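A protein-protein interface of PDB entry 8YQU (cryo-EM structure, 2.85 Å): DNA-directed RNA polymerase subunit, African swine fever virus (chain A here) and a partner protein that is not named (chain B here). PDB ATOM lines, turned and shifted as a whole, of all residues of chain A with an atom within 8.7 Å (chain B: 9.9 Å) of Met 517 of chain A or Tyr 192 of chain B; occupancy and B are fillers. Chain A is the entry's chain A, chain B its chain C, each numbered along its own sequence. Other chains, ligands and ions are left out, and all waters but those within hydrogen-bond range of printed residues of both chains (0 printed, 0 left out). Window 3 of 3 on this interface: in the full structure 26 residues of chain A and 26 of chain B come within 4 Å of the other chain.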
ATOM      1  N   ARG A 512      18.762 -29.207 -39.241  1.00  0.00           N
ATOM      2  CA  ARG A 512      19.252 -28.311 -38.204  1.00  0.00           C
ATOM      3  C   ARG A 512      19.484 -29.075 -36.906  1.00  0.00           C
ATOM      4  O   ARG A 512      18.731 -29.987 -36.560  1.00  0.00           O
ATOM      5  CB  ARG A 512      18.248 -27.178 -37.994  1.00  0.00           C
ATOM      6  CG  ARG A 512      18.631 -26.136 -36.973  1.00  0.00           C
ATOM      7  CD  ARG A 512      17.532 -25.095 -36.876  1.00  0.00           C
ATOM      8  NE  ARG A 512      16.218 -25.717 -36.769  1.00  0.00           N
ATOM      9  CZ  ARG A 512      15.078 -25.050 -36.660  1.00  0.00           C
ATOM     10  NH1 ARG A 512      15.051 -23.729 -36.629  1.00  0.00           N
ATOM     11  NH2 ARG A 512      13.936 -25.727 -36.577  1.00  0.00           N
ATOM     12  N   THR A 513      20.546 -28.703 -36.189  1.00  0.00           N
ATOM     13  CA  THR A 513      20.926 -29.438 -34.987  1.00  0.00           C
ATOM     14  C   THR A 513      20.032 -29.086 -33.803  1.00  0.00           C
ATOM     15  O   THR A 513      19.536 -29.975 -33.104  1.00  0.00           O
ATOM     16  CB  THR A 513      22.390 -29.165 -34.644  1.00  0.00           C
ATOM     17  OG1 THR A 513      23.222 -29.578 -35.736  1.00  0.00           O
ATOM     18  CG2 THR A 513      22.796 -29.923 -33.393  1.00  0.00           C
ATOM     19  N   ASN A 514      19.814 -27.796 -33.563  1.00  0.00           N
ATOM     20  CA  ASN A 514      19.030 -27.331 -32.431  1.00  0.00           C
ATOM     21  C   ASN A 514      17.852 -26.500 -32.915  1.00  0.00           C
ATOM     22  O   ASN A 514      17.998 -25.648 -33.796  1.00  0.00           O
ATOM     23  CB  ASN A 514      19.885 -26.504 -31.465  1.00  0.00           C
ATOM     24  CG  ASN A 514      20.962 -27.326 -30.790  1.00  0.00           C
ATOM     25  OD1 ASN A 514      22.153 -27.066 -30.958  1.00  0.00           O
ATOM     26  ND2 ASN A 514      20.550 -28.325 -30.020  1.00  0.00           N
ATOM     27  N   THR A 515      16.707 -26.746 -32.333  1.00  0.00           N
ATOM     28  CA  THR A 515      15.381 -26.167 -32.452  1.00  0.00           C
ATOM     29  C   THR A 515      15.121 -25.222 -31.282  1.00  0.00           C
ATOM     30  O   THR A 515      15.625 -25.445 -30.178  1.00  0.00           O
ATOM     31  CB  THR A 515      14.326 -27.284 -32.475  1.00  0.00           C
ATOM     32  OG1 THR A 515      14.544 -28.120 -33.617  1.00  0.00           O
ATOM     33  CG2 THR A 515      12.908 -26.737 -32.530  1.00  0.00           C
ATOM     34  N   PRO A 516      14.362 -24.131 -31.477  1.00  0.00           N
ATOM     35  CA  PRO A 516      14.023 -23.259 -30.342  1.00  0.00           C
ATOM     36  C   PRO A 516      13.299 -23.974 -29.209  1.00  0.00           C
ATOM     37  O   PRO A 516      13.067 -23.385 -28.149  1.00  0.00           O
ATOM     38  CB  PRO A 516      13.129 -22.193 -30.984  1.00  0.00           C
ATOM     39  CG  PRO A 516      13.603 -22.118 -32.384  1.00  0.00           C
ATOM     40  CD  PRO A 516      14.018 -23.509 -32.769  1.00  0.00           C
ATOM     41  N   MET A 517      12.940 -25.238 -29.416  1.00  0.00           N
ATOM     42  CA  MET A 517      12.272 -26.058 -28.414  1.00  0.00           C
ATOM     43  C   MET A 517      13.155 -27.239 -28.020  1.00  0.00           C
ATOM     44  O   MET A 517      12.674 -28.338 -27.734  1.00  0.00           O
ATOM     45  CB  MET A 517      10.913 -26.529 -28.930  1.00  0.00           C
ATOM     46  CG  MET A 517       9.944 -26.987 -27.853  1.00  0.00           C
ATOM     47  SD  MET A 517       9.054 -25.598 -27.133  1.00  0.00           S
ATOM     48  CE  MET A 517       8.045 -25.099 -28.526  1.00  0.00           C
ATOM     49  N   GLY A 518      14.463 -27.025 -28.008  1.00  0.00           N
ATOM     50  CA  GLY A 518      15.410 -28.054 -27.630  1.00  0.00           C
ATOM     51  C   GLY A 518      16.110 -28.684 -28.817  1.00  0.00           C
ATOM     52  O   GLY A 518      16.207 -28.114 -29.907  1.00  0.00           O
ATOM     53  N   LYS A 519      16.612 -29.893 -28.589  1.00  0.00           N
ATOM     54  CA  LYS A 519      17.296 -30.627 -29.642  1.00  0.00           C
ATOM     55  C   LYS A 519      16.311 -31.036 -30.733  1.00  0.00           C
ATOM     56  O   LYS A 519      15.153 -31.368 -30.465  1.00  0.00           O
ATOM     57  CB  LYS A 519      17.995 -31.859 -29.065  1.00  0.00           C
ATOM     58  CG  LYS A 519      18.789 -32.660 -30.082  1.00  0.00           C
ATOM     59  CD  LYS A 519      19.552 -33.797 -29.425  1.00  0.00           C
ATOM     60  CE  LYS A 519      20.214 -34.687 -30.465  1.00  0.00           C
ATOM     61  NZ  LYS A 519      21.278 -33.971 -31.221  1.00  0.00           N
ATOM     62  N   ASN A 520      16.787 -31.010 -31.978  1.00  0.00           N
ATOM     63  CA  ASN A 520      15.948 -31.298 -33.142  1.00  0.00           C
ATOM     64  C   ASN A 520      15.825 -32.810 -33.302  1.00  0.00           C
ATOM     65  O   ASN A 520      16.500 -33.445 -34.114  1.00  0.00           O
ATOM     66  CB  ASN A 520      16.526 -30.644 -34.390  1.00  0.00           C
ATOM     67  CG  ASN A 520      15.521 -30.558 -35.519  1.00  0.00           C
ATOM     68  OD1 ASN A 520      14.357 -30.919 -35.358  1.00  0.00           O
ATOM     69  ND2 ASN A 520      15.969 -30.079 -36.672  1.00  0.00           N
ATOM     70  N   VAL A 521      14.931 -33.393 -32.503  1.00  0.00           N
ATOM     71  CA  VAL A 521      14.655 -34.821 -32.536  1.00  0.00           C
ATOM     72  C   VAL A 521      13.157 -35.027 -32.718  1.00  0.00           C
ATOM     73  O   VAL A 521      12.356 -34.100 -32.601  1.00  0.00           O
ATOM     74  CB  VAL A 521      15.150 -35.547 -31.269  1.00  0.00           C
ATOM     75  CG1 VAL A 521      16.660 -35.455 -31.162  1.00  0.00           C
ATOM     76  CG2 VAL A 521      14.486 -34.965 -30.034  1.00  0.00           C
ATOM     77  N   ALA A 647       6.294 -28.557 -38.000  1.00  0.00           N
ATOM     78  CA  ALA A 647       7.322 -27.650 -37.511  1.00  0.00           C
ATOM     79  C   ALA A 647       7.025 -26.197 -37.834  1.00  0.00           C
ATOM     80  O   ALA A 647       7.429 -25.308 -37.079  1.00  0.00           O
ATOM     81  CB  ALA A 647       8.689 -28.025 -38.093  1.00  0.00           C
ATOM     82  N   GLU A 726      17.242 -18.075 -35.088  1.00  0.00           N
ATOM     83  CA  GLU A 726      16.643 -19.388 -34.904  1.00  0.00           C
ATOM     84  C   GLU A 726      15.139 -19.395 -35.137  1.00  0.00           C
ATOM     85  O   GLU A 726      14.559 -20.474 -35.295  1.00  0.00           O
ATOM     86  CB  GLU A 726      16.949 -19.906 -33.497  1.00  0.00           C
ATOM     87  CG  GLU A 726      17.166 -21.406 -33.423  1.00  0.00           C
ATOM     88  CD  GLU A 726      17.854 -21.829 -32.143  1.00  0.00           C
ATOM     89  OE1 GLU A 726      18.057 -20.966 -31.263  1.00  0.00           O
ATOM     90  OE2 GLU A 726      18.196 -23.023 -32.016  1.00  0.00           O
ATOM     91  N   THR A 727      14.493 -18.226 -35.165  1.00  0.00           N
ATOM     92  CA  THR A 727      13.054 -18.144 -35.376  1.00  0.00           C
ATOM     93  C   THR A 727      12.637 -17.180 -36.478  1.00  0.00           C
ATOM     94  O   THR A 727      11.458 -17.177 -36.845  1.00  0.00           O
ATOM     95  CB  THR A 727      12.335 -17.729 -34.081  1.00  0.00           C
ATOM     96  OG1 THR A 727      12.690 -16.383 -33.744  1.00  0.00           O
ATOM     97  CG2 THR A 727      12.704 -18.649 -32.932  1.00  0.00           C
ATOM     98  N   ILE B 189      -0.503 -30.452 -21.670  1.00  0.00           N
ATOM     99  CA  ILE B 189       0.770 -29.873 -22.081  1.00  0.00           C
ATOM    100  C   ILE B 189       0.829 -28.444 -21.561  1.00  0.00           C
ATOM    101  O   ILE B 189      -0.111 -27.667 -21.761  1.00  0.00           O
ATOM    102  CB  ILE B 189       0.950 -29.902 -23.610  1.00  0.00           C
ATOM    103  CG1 ILE B 189       0.728 -31.313 -24.153  1.00  0.00           C
ATOM    104  CG2 ILE B 189       2.337 -29.414 -23.989  1.00  0.00           C
ATOM    105  CD1 ILE B 189       0.808 -31.396 -25.659  1.00  0.00           C
ATOM    106  N   GLU B 190       1.927 -28.103 -20.892  1.00  0.00           N
ATOM    107  CA  GLU B 190       2.102 -26.753 -20.385  1.00  0.00           C
ATOM    108  C   GLU B 190       2.369 -25.784 -21.533  1.00  0.00           C
ATOM    109  O   GLU B 190       2.776 -26.173 -22.630  1.00  0.00           O
ATOM    110  CB  GLU B 190       3.246 -26.704 -19.373  1.00  0.00           C
ATOM    111  CG  GLU B 190       2.978 -27.489 -18.102  1.00  0.00           C
ATOM    112  CD  GLU B 190       1.854 -26.894 -17.277  1.00  0.00           C
ATOM    113  OE1 GLU B 190       1.683 -25.658 -17.302  1.00  0.00           O
ATOM    114  OE2 GLU B 190       1.137 -27.665 -16.604  1.00  0.00           O
ATOM    115  N   GLN B 191       2.134 -24.500 -21.267  1.00  0.00           N
ATOM    116  CA  GLN B 191       2.256 -23.464 -22.281  1.00  0.00           C
ATOM    117  C   GLN B 191       3.110 -22.316 -21.767  1.00  0.00           C
ATOM    118  O   GLN B 191       3.054 -21.969 -20.583  1.00  0.00           O
ATOM    119  CB  GLN B 191       0.880 -22.933 -22.699  1.00  0.00           C
ATOM    120  CG  GLN B 191      -0.029 -23.975 -23.321  1.00  0.00           C
ATOM    121  CD  GLN B 191      -1.293 -23.371 -23.896  1.00  0.00           C
ATOM    122  OE1 GLN B 191      -1.455 -22.152 -23.924  1.00  0.00           O
ATOM    123  NE2 GLN B 191      -2.199 -24.224 -24.359  1.00  0.00           N
ATOM    124  N   TYR B 192       3.901 -21.731 -22.664  1.00  0.00           N
ATOM    125  CA  TYR B 192       4.631 -20.520 -22.336  1.00  0.00           C
ATOM    126  C   TYR B 192       3.686 -19.321 -22.321  1.00  0.00           C
ATOM    127  O   TYR B 192       2.647 -19.330 -22.987  1.00  0.00           O
ATOM    128  CB  TYR B 192       5.742 -20.256 -23.350  1.00  0.00           C
ATOM    129  CG  TYR B 192       6.860 -21.268 -23.374  1.00  0.00           C
ATOM    130  CD1 TYR B 192       7.668 -21.468 -22.263  1.00  0.00           C
ATOM    131  CD2 TYR B 192       7.129 -22.002 -24.520  1.00  0.00           C
ATOM    132  CE1 TYR B 192       8.698 -22.384 -22.288  1.00  0.00           C
ATOM    133  CE2 TYR B 192       8.157 -22.919 -24.554  1.00  0.00           C
ATOM    134  CZ  TYR B 192       8.939 -23.107 -23.437  1.00  0.00           C
ATOM    135  OH  TYR B 192       9.964 -24.023 -23.470  1.00  0.00           O
ATOM    136  N   PRO B 193       4.021 -18.275 -21.570  1.00  0.00           N
ATOM    137  CA  PRO B 193       3.328 -16.995 -21.758  1.00  0.00           C
ATOM    138  C   PRO B 193       3.793 -16.325 -23.040  1.00  0.00           C
ATOM    139  O   PRO B 193       4.909 -15.801 -23.101  1.00  0.00           O
ATOM    140  CB  PRO B 193       3.726 -16.186 -20.515  1.00  0.00           C
ATOM    141  CG  PRO B 193       4.275 -17.199 -19.545  1.00  0.00           C
ATOM    142  CD  PRO B 193       4.907 -18.249 -20.396  1.00  0.00           C
ATOM    143  N   THR B 194       2.949 -16.334 -24.069  1.00  0.00           N
ATOM    144  CA  THR B 194       3.350 -15.848 -25.383  1.00  0.00           C
ATOM    145  C   THR B 194       3.260 -14.333 -25.511  1.00  0.00           C
ATOM    146  O   THR B 194       3.619 -13.797 -26.564  1.00  0.00           O
ATOM    147  CB  THR B 194       2.500 -16.506 -26.472  1.00  0.00           C
ATOM    148  OG1 THR B 194       1.117 -16.453 -26.102  1.00  0.00           O
ATOM    149  CG2 THR B 194       2.914 -17.957 -26.659  1.00  0.00           C
ATOM    150  N   ASP B 195       2.788 -13.637 -24.476  1.00  0.00           N
ATOM    151  CA  ASP B 195       2.812 -12.180 -24.496  1.00  0.00           C
ATOM    152  C   ASP B 195       4.237 -11.650 -24.531  1.00  0.00           C
ATOM    153  O   ASP B 195       4.493 -10.594 -25.120  1.00  0.00           O
ATOM    154  CB  ASP B 195       2.069 -11.628 -23.280  1.00  0.00           C
ATOM    155  CG  ASP B 195       0.642 -12.127 -23.196  1.00  0.00           C
ATOM    156  OD1 ASP B 195       0.038 -12.379 -24.261  1.00  0.00           O
ATOM    157  OD2 ASP B 195       0.127 -12.273 -22.069  1.00  0.00           O
ATOM    158  N   LYS B 196       5.171 -12.364 -23.910  1.00  0.00           N
ATOM    159  CA  LYS B 196       6.564 -11.948 -23.908  1.00  0.00           C
ATOM    160  C   LYS B 196       7.150 -12.033 -25.314  1.00  0.00           C
ATOM    161  O   LYS B 196       6.818 -12.927 -26.097  1.00  0.00           O
ATOM    162  CB  LYS B 196       7.375 -12.818 -22.950  1.00  0.00           C
ATOM    163  CG  LYS B 196       6.881 -12.772 -21.516  1.00  0.00           C
ATOM    164  CD  LYS B 196       7.051 -11.390 -20.914  1.00  0.00           C
ATOM    165  CE  LYS B 196       6.702 -11.388 -19.435  1.00  0.00           C
ATOM    166  NZ  LYS B 196       5.244 -11.595 -19.216  1.00  0.00           N
ATOM    167  N   LYS B 197       8.034 -11.087 -25.629  1.00  0.00           N
ATOM    168  CA  LYS B 197       8.666 -11.052 -26.941  1.00  0.00           C
ATOM    169  C   LYS B 197       9.650 -12.193 -27.157  1.00  0.00           C
ATOM    170  O   LYS B 197      10.034 -12.449 -28.303  1.00  0.00           O
ATOM    171  CB  LYS B 197       9.379  -9.713 -27.145  1.00  0.00           C
ATOM    172  CG  LYS B 197       8.454  -8.585 -27.572  1.00  0.00           C
ATOM    173  CD  LYS B 197       9.096  -7.712 -28.635  1.00  0.00           C
ATOM    174  CE  LYS B 197       8.265  -6.468 -28.893  1.00  0.00           C
ATOM    175  NZ  LYS B 197       8.342  -5.506 -27.759  1.00  0.00           N
ATOM    176  N   GLU B 198      10.063 -12.881 -26.091  1.00  0.00           N
ATOM    177  CA  GLU B 198      10.942 -14.034 -26.226  1.00  0.00           C
ATOM    178  C   GLU B 198      10.221 -15.259 -26.770  1.00  0.00           C
ATOM    179  O   GLU B 198      10.860 -16.112 -27.396  1.00  0.00           O
ATOM    180  CB  GLU B 198      11.570 -14.370 -24.870  1.00  0.00           C
ATOM    181  CG  GLU B 198      12.573 -15.512 -24.904  1.00  0.00           C
ATOM    182  CD  GLU B 198      13.191 -15.783 -23.548  1.00  0.00           C
ATOM    183  OE1 GLU B 198      12.823 -15.092 -22.577  1.00  0.00           O
ATOM    184  OE2 GLU B 198      14.042 -16.693 -23.454  1.00  0.00           O
ATOM    185  N   TYR B 199       8.910 -15.354 -26.566  1.00  0.00           N
ATOM    186  CA  TYR B 199       8.157 -16.551 -26.906  1.00  0.00           C
ATOM    187  C   TYR B 199       7.074 -16.317 -27.947  1.00  0.00           C
ATOM    188  O   TYR B 199       6.363 -17.266 -28.296  1.00  0.00           O
ATOM    189  CB  TYR B 199       7.517 -17.143 -25.644  1.00  0.00           C
ATOM    190  CG  TYR B 199       8.511 -17.682 -24.643  1.00  0.00           C
ATOM    191  CD1 TYR B 199       9.656 -18.345 -25.061  1.00  0.00           C
ATOM    192  CD2 TYR B 199       8.306 -17.524 -23.281  1.00  0.00           C
ATOM    193  CE1 TYR B 199      10.567 -18.837 -24.148  1.00  0.00           C
ATOM    194  CE2 TYR B 199       9.212 -18.013 -22.361  1.00  0.00           C
ATOM    195  CZ  TYR B 199      10.340 -18.669 -22.800  1.00  0.00           C
ATOM    196  OH  TYR B 199      11.245 -19.158 -21.886  1.00  0.00           O
ATOM    197  N   MET B 200       6.920 -15.093 -28.454  1.00  0.00           N
ATOM    198  CA  MET B 200       5.823 -14.810 -29.371  1.00  0.00           C
ATOM    199  C   MET B 200       6.015 -15.443 -30.742  1.00  0.00           C
ATOM    200  O   MET B 200       5.051 -15.513 -31.511  1.00  0.00           O
ATOM    201  CB  MET B 200       5.631 -13.301 -29.526  1.00  0.00           C
ATOM    202  CG  MET B 200       6.843 -12.565 -30.061  1.00  0.00           C
ATOM    203  SD  MET B 200       6.607 -10.779 -30.054  1.00  0.00           S
ATOM    204  CE  MET B 200       7.675 -10.292 -31.406  1.00  0.00           C
ATOM    205  N   ALA B 201       7.221 -15.902 -31.068  1.00  0.00           N
ATOM    206  CA  ALA B 201       7.467 -16.571 -32.336  1.00  0.00           C
ATOM    207  C   ALA B 201       7.193 -18.066 -32.279  1.00  0.00           C
ATOM    208  O   ALA B 201       7.215 -18.725 -33.325  1.00  0.00           O
ATOM    209  CB  ALA B 201       8.910 -16.335 -32.789  1.00  0.00           C
ATOM    210  N   LEU B 202       6.935 -18.612 -31.097  1.00  0.00           N
ATOM    211  CA  LEU B 202       6.646 -20.026 -30.920  1.00  0.00           C
ATOM    212  C   LEU B 202       5.146 -20.240 -30.758  1.00  0.00           C
ATOM    213  O   LEU B 202       4.375 -19.301 -30.550  1.00  0.00           O
ATOM    214  CB  LEU B 202       7.400 -20.579 -29.708  1.00  0.00           C
ATOM    215  CG  LEU B 202       8.866 -20.168 -29.553  1.00  0.00           C
ATOM    216  CD1 LEU B 202       9.492 -20.874 -28.365  1.00  0.00           C
ATOM    217  CD2 LEU B 202       9.647 -20.463 -30.823  1.00  0.00           C
ATOM    218  N   SER B 203       4.734 -21.505 -30.866  1.00  0.00           N
ATOM    219  CA  SER B 203       3.322 -21.830 -30.688  1.00  0.00           C
ATOM    220  C   SER B 203       2.866 -21.532 -29.267  1.00  0.00           C
ATOM    221  O   SER B 203       1.789 -20.963 -29.058  1.00  0.00           O
ATOM    222  CB  SER B 203       3.072 -23.298 -31.030  1.00  0.00           C
ATOM    223  OG  SER B 203       3.559 -24.147 -30.006  1.00  0.00           O
ATOM    224  N   GLY B 204       3.678 -21.897 -28.279  1.00  0.00           N
ATOM    225  CA  GLY B 204       3.324 -21.679 -26.893  1.00  0.00           C
ATOM    226  C   GLY B 204       3.497 -22.921 -26.044  1.00  0.00           C
ATOM    227  O   GLY B 204       3.910 -22.830 -24.886  1.00  0.00           O
ATOM    228  N   TYR B 205       3.190 -24.085 -26.612  1.00  0.00           N
ATOM    229  CA  TYR B 205       3.343 -25.336 -25.883  1.00  0.00           C
ATOM    230  C   TYR B 205       4.807 -25.580 -25.543  1.00  0.00           C
ATOM    231  O   TYR B 205       5.707 -25.236 -26.313  1.00  0.00           O
ATOM    232  CB  TYR B 205       2.795 -26.503 -26.705  1.00  0.00           C
ATOM    233  CG  TYR B 205       1.288 -26.537 -26.802  1.00  0.00           C
ATOM    234  CD1 TYR B 205       0.509 -26.846 -25.697  1.00  0.00           C
ATOM    235  CD2 TYR B 205       0.646 -26.273 -28.004  1.00  0.00           C
ATOM    236  CE1 TYR B 205      -0.868 -26.883 -25.783  1.00  0.00           C
ATOM    237  CE2 TYR B 205      -0.730 -26.309 -28.098  1.00  0.00           C
ATOM    238  CZ  TYR B 205      -1.481 -26.613 -26.986  1.00  0.00           C
ATOM    239  OH  TYR B 205      -2.852 -26.648 -27.075  1.00  0.00           O
ATOM    240  N   LYS B 206       5.044 -26.178 -24.378  1.00  0.00           N
ATOM    241  CA  LYS B 206       6.401 -26.436 -23.916  1.00  0.00           C
ATOM    242  C   LYS B 206       6.982 -27.733 -24.460  1.00  0.00           C
ATOM    243  O   LYS B 206       8.138 -28.047 -24.160  1.00  0.00           O
ATOM    244  CB  LYS B 206       6.440 -26.454 -22.386  1.00  0.00           C
ATOM    245  CG  LYS B 206       6.292 -25.081 -21.758  1.00  0.00           C
ATOM    246  CD  LYS B 206       6.508 -25.129 -20.259  1.00  0.00           C
ATOM    247  CE  LYS B 206       6.407 -23.743 -19.649  1.00  0.00           C
ATOM    248  NZ  LYS B 206       6.654 -23.759 -18.182  1.00  0.00           N
ATOM    249  N   GLN B 207       6.219 -28.491 -25.243  1.00  0.00           N
ATOM    250  CA  GLN B 207       6.706 -29.704 -25.882  1.00  0.00           C
ATOM    251  C   GLN B 207       6.503 -29.599 -27.386  1.00  0.00           C
ATOM    252  O   GLN B 207       5.455 -29.142 -27.850  1.00  0.00           O
ATOM    253  CB  GLN B 207       5.987 -30.943 -25.346  1.00  0.00           C
ATOM    254  CG  GLN B 207       6.197 -31.192 -23.866  1.00  0.00           C
ATOM    255  CD  GLN B 207       5.392 -32.368 -23.360  1.00  0.00           C
ATOM    256  OE1 GLN B 207       4.660 -33.006 -24.116  1.00  0.00           O
ATOM    257  NE2 GLN B 207       5.520 -32.663 -22.072  1.00  0.00           N
ATOM    258  N   SER B 208       7.510 -30.024 -28.142  1.00  0.00           N
ATOM    259  CA  SER B 208       7.414 -30.007 -29.593  1.00  0.00           C
ATOM    260  C   SER B 208       6.402 -31.040 -30.076  1.00  0.00           C
ATOM    261  O   SER B 208       6.222 -32.099 -29.468  1.00  0.00           O
ATOM    262  CB  SER B 208       8.779 -30.279 -30.222  1.00  0.00           C
ATOM    263  OG  SER B 208       8.713 -30.207 -31.634  1.00  0.00           O
ATOM    264  N   SER B 209       5.731 -30.720 -31.184  1.00  0.00           N
ATOM    265  CA  SER B 209       4.774 -31.654 -31.763  1.00  0.00           C
ATOM    266  C   SER B 209       5.448 -32.911 -32.294  1.00  0.00           C
ATOM    267  O   SER B 209       4.781 -33.938 -32.447  1.00  0.00           O
ATOM    268  CB  SER B 209       3.984 -30.978 -32.882  1.00  0.00           C
ATOM    269  OG  SER B 209       4.834 -30.575 -33.938  1.00  0.00           O
ATOM    270  N   MET B 210       6.750 -32.849 -32.578  1.00  0.00           N
ATOM    271  CA  MET B 210       7.508 -34.025 -32.981  1.00  0.00           C
ATOM    272  C   MET B 210       7.706 -35.025 -31.850  1.00  0.00           C
ATOM    273  O   MET B 210       8.151 -36.145 -32.116  1.00  0.00           O
ATOM    274  CB  MET B 210       8.874 -33.608 -33.527  1.00  0.00           C
ATOM    275  CG  MET B 210       8.855 -32.999 -34.917  1.00  0.00           C
ATOM    276  SD  MET B 210       8.578 -34.261 -36.174  1.00  0.00           S
ATOM    277  CE  MET B 210       8.746 -33.305 -37.673  1.00  0.00           C
ATOM    278  N   THR B 211       7.404 -34.655 -30.607  1.00  0.00           N
ATOM    279  CA  THR B 211       7.666 -35.540 -29.479  1.00  0.00           C
ATOM    280  C   THR B 211       6.433 -35.723 -28.602  1.00  0.00           C
ATOM    281  O   THR B 211       6.254 -36.779 -27.988  1.00  0.00           O
ATOM    282  CB  THR B 211       8.829 -34.998 -28.644  1.00  0.00           C
ATOM    283  OG1 THR B 211       9.900 -34.607 -29.511  1.00  0.00           O
ATOM    284  CG2 THR B 211       9.336 -36.059 -27.679  1.00  0.00           C
ATOM    285  N   SER B 212       5.577 -34.707 -28.541  1.00  0.00           N
ATOM    286  CA  SER B 212       4.449 -34.736 -27.622  1.00  0.00           C
ATOM    287  C   SER B 212       3.386 -35.730 -28.083  1.00  0.00           C
ATOM    288  O   SER B 212       3.191 -35.972 -29.276  1.00  0.00           O
ATOM    289  CB  SER B 212       3.836 -33.344 -27.487  1.00  0.00           C
ATOM    290  OG  SER B 212       3.187 -32.957 -28.685  1.00  0.00           O
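The backbone carbonyl oxygen of Tyr 205 of chain B lies close to the side-chain sulfur of Met 517 of chain A (3.5 Å).
The backbone carbonyl oxygen (O) of Glu 190 of chain B is in hydrogen-bond range of the backbone NH (N) of Lys 206 of chain B (2.9 Å).
N of Tyr 192 of chain B lies within hydrogen-bond range of O of Gly 204 of chain B, at 2.5 Å.
N of Tyr 205 of chain B lies within hydrogen-bond range of OG of Ser 203 of chain B, at 3.4 Å.
The backbone NH (N) of Met 210 of chain B lies close to the side-chain hydroxyl (OG) of Ser 208 of chain B.
The backbone carbonyl oxygen (O) of Ser 208 of chain B is in hydrogen-bond range of the side-chain hydroxyl (OG) of Ser 212 of chain B (3.2 Å).
Leu 202 of chain B touches Pro 516 of chain A.
Met 517 of chain A touches Tyr 192 of chain B (SD to CE2, 3.8 Å).
Met 517 of chain A touches Lys 206 of chain B (SD to O, 3.96 Å).
Met 517 of chain A touches Ser 208 of chain B (CG to N, 3.9 Å).
CB of Met 210 of chain B touches O of Val 521 of chain A (3.6 Å).
Val 521 of chain A touches Thr 211 of chain B (O to OG1, 3.98 Å).
Ala 201 of chain B touches Thr 727 of chain A.
Pro 516 of chain A touches just one residue of chain B: Leu 202.
Met 517 of chain A touches just these residues of chain B: Tyr 192, Tyr 205, Lys 206 and Ser 208.
No residue of chain B comes within 4 Å of Gly 518 of chain A.
Lys 519 of chain A touches none of the printed residues of chain B.
Printed residues of chain B within 4 Å of Thr 727 of chain A: Ala 201 (3.9 Å).
Of the printed residues of chain A, Tyr 192 of chain B touches Met 517 (3.8 Å).
No residue of chain A comes within 4 Å of Pro 193 of chain B.
Printed residues of chain A within 4 Å of Tyr 205 of chain B: Met 517.
The nearest residue of chain A that does not touch Tyr 192 of chain B is Pro 516 of chain A (5.7 Å).
Hydrophobic or aromatic side chains of chain A that line the printed part of chain B: Pro 516 and Met 517.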
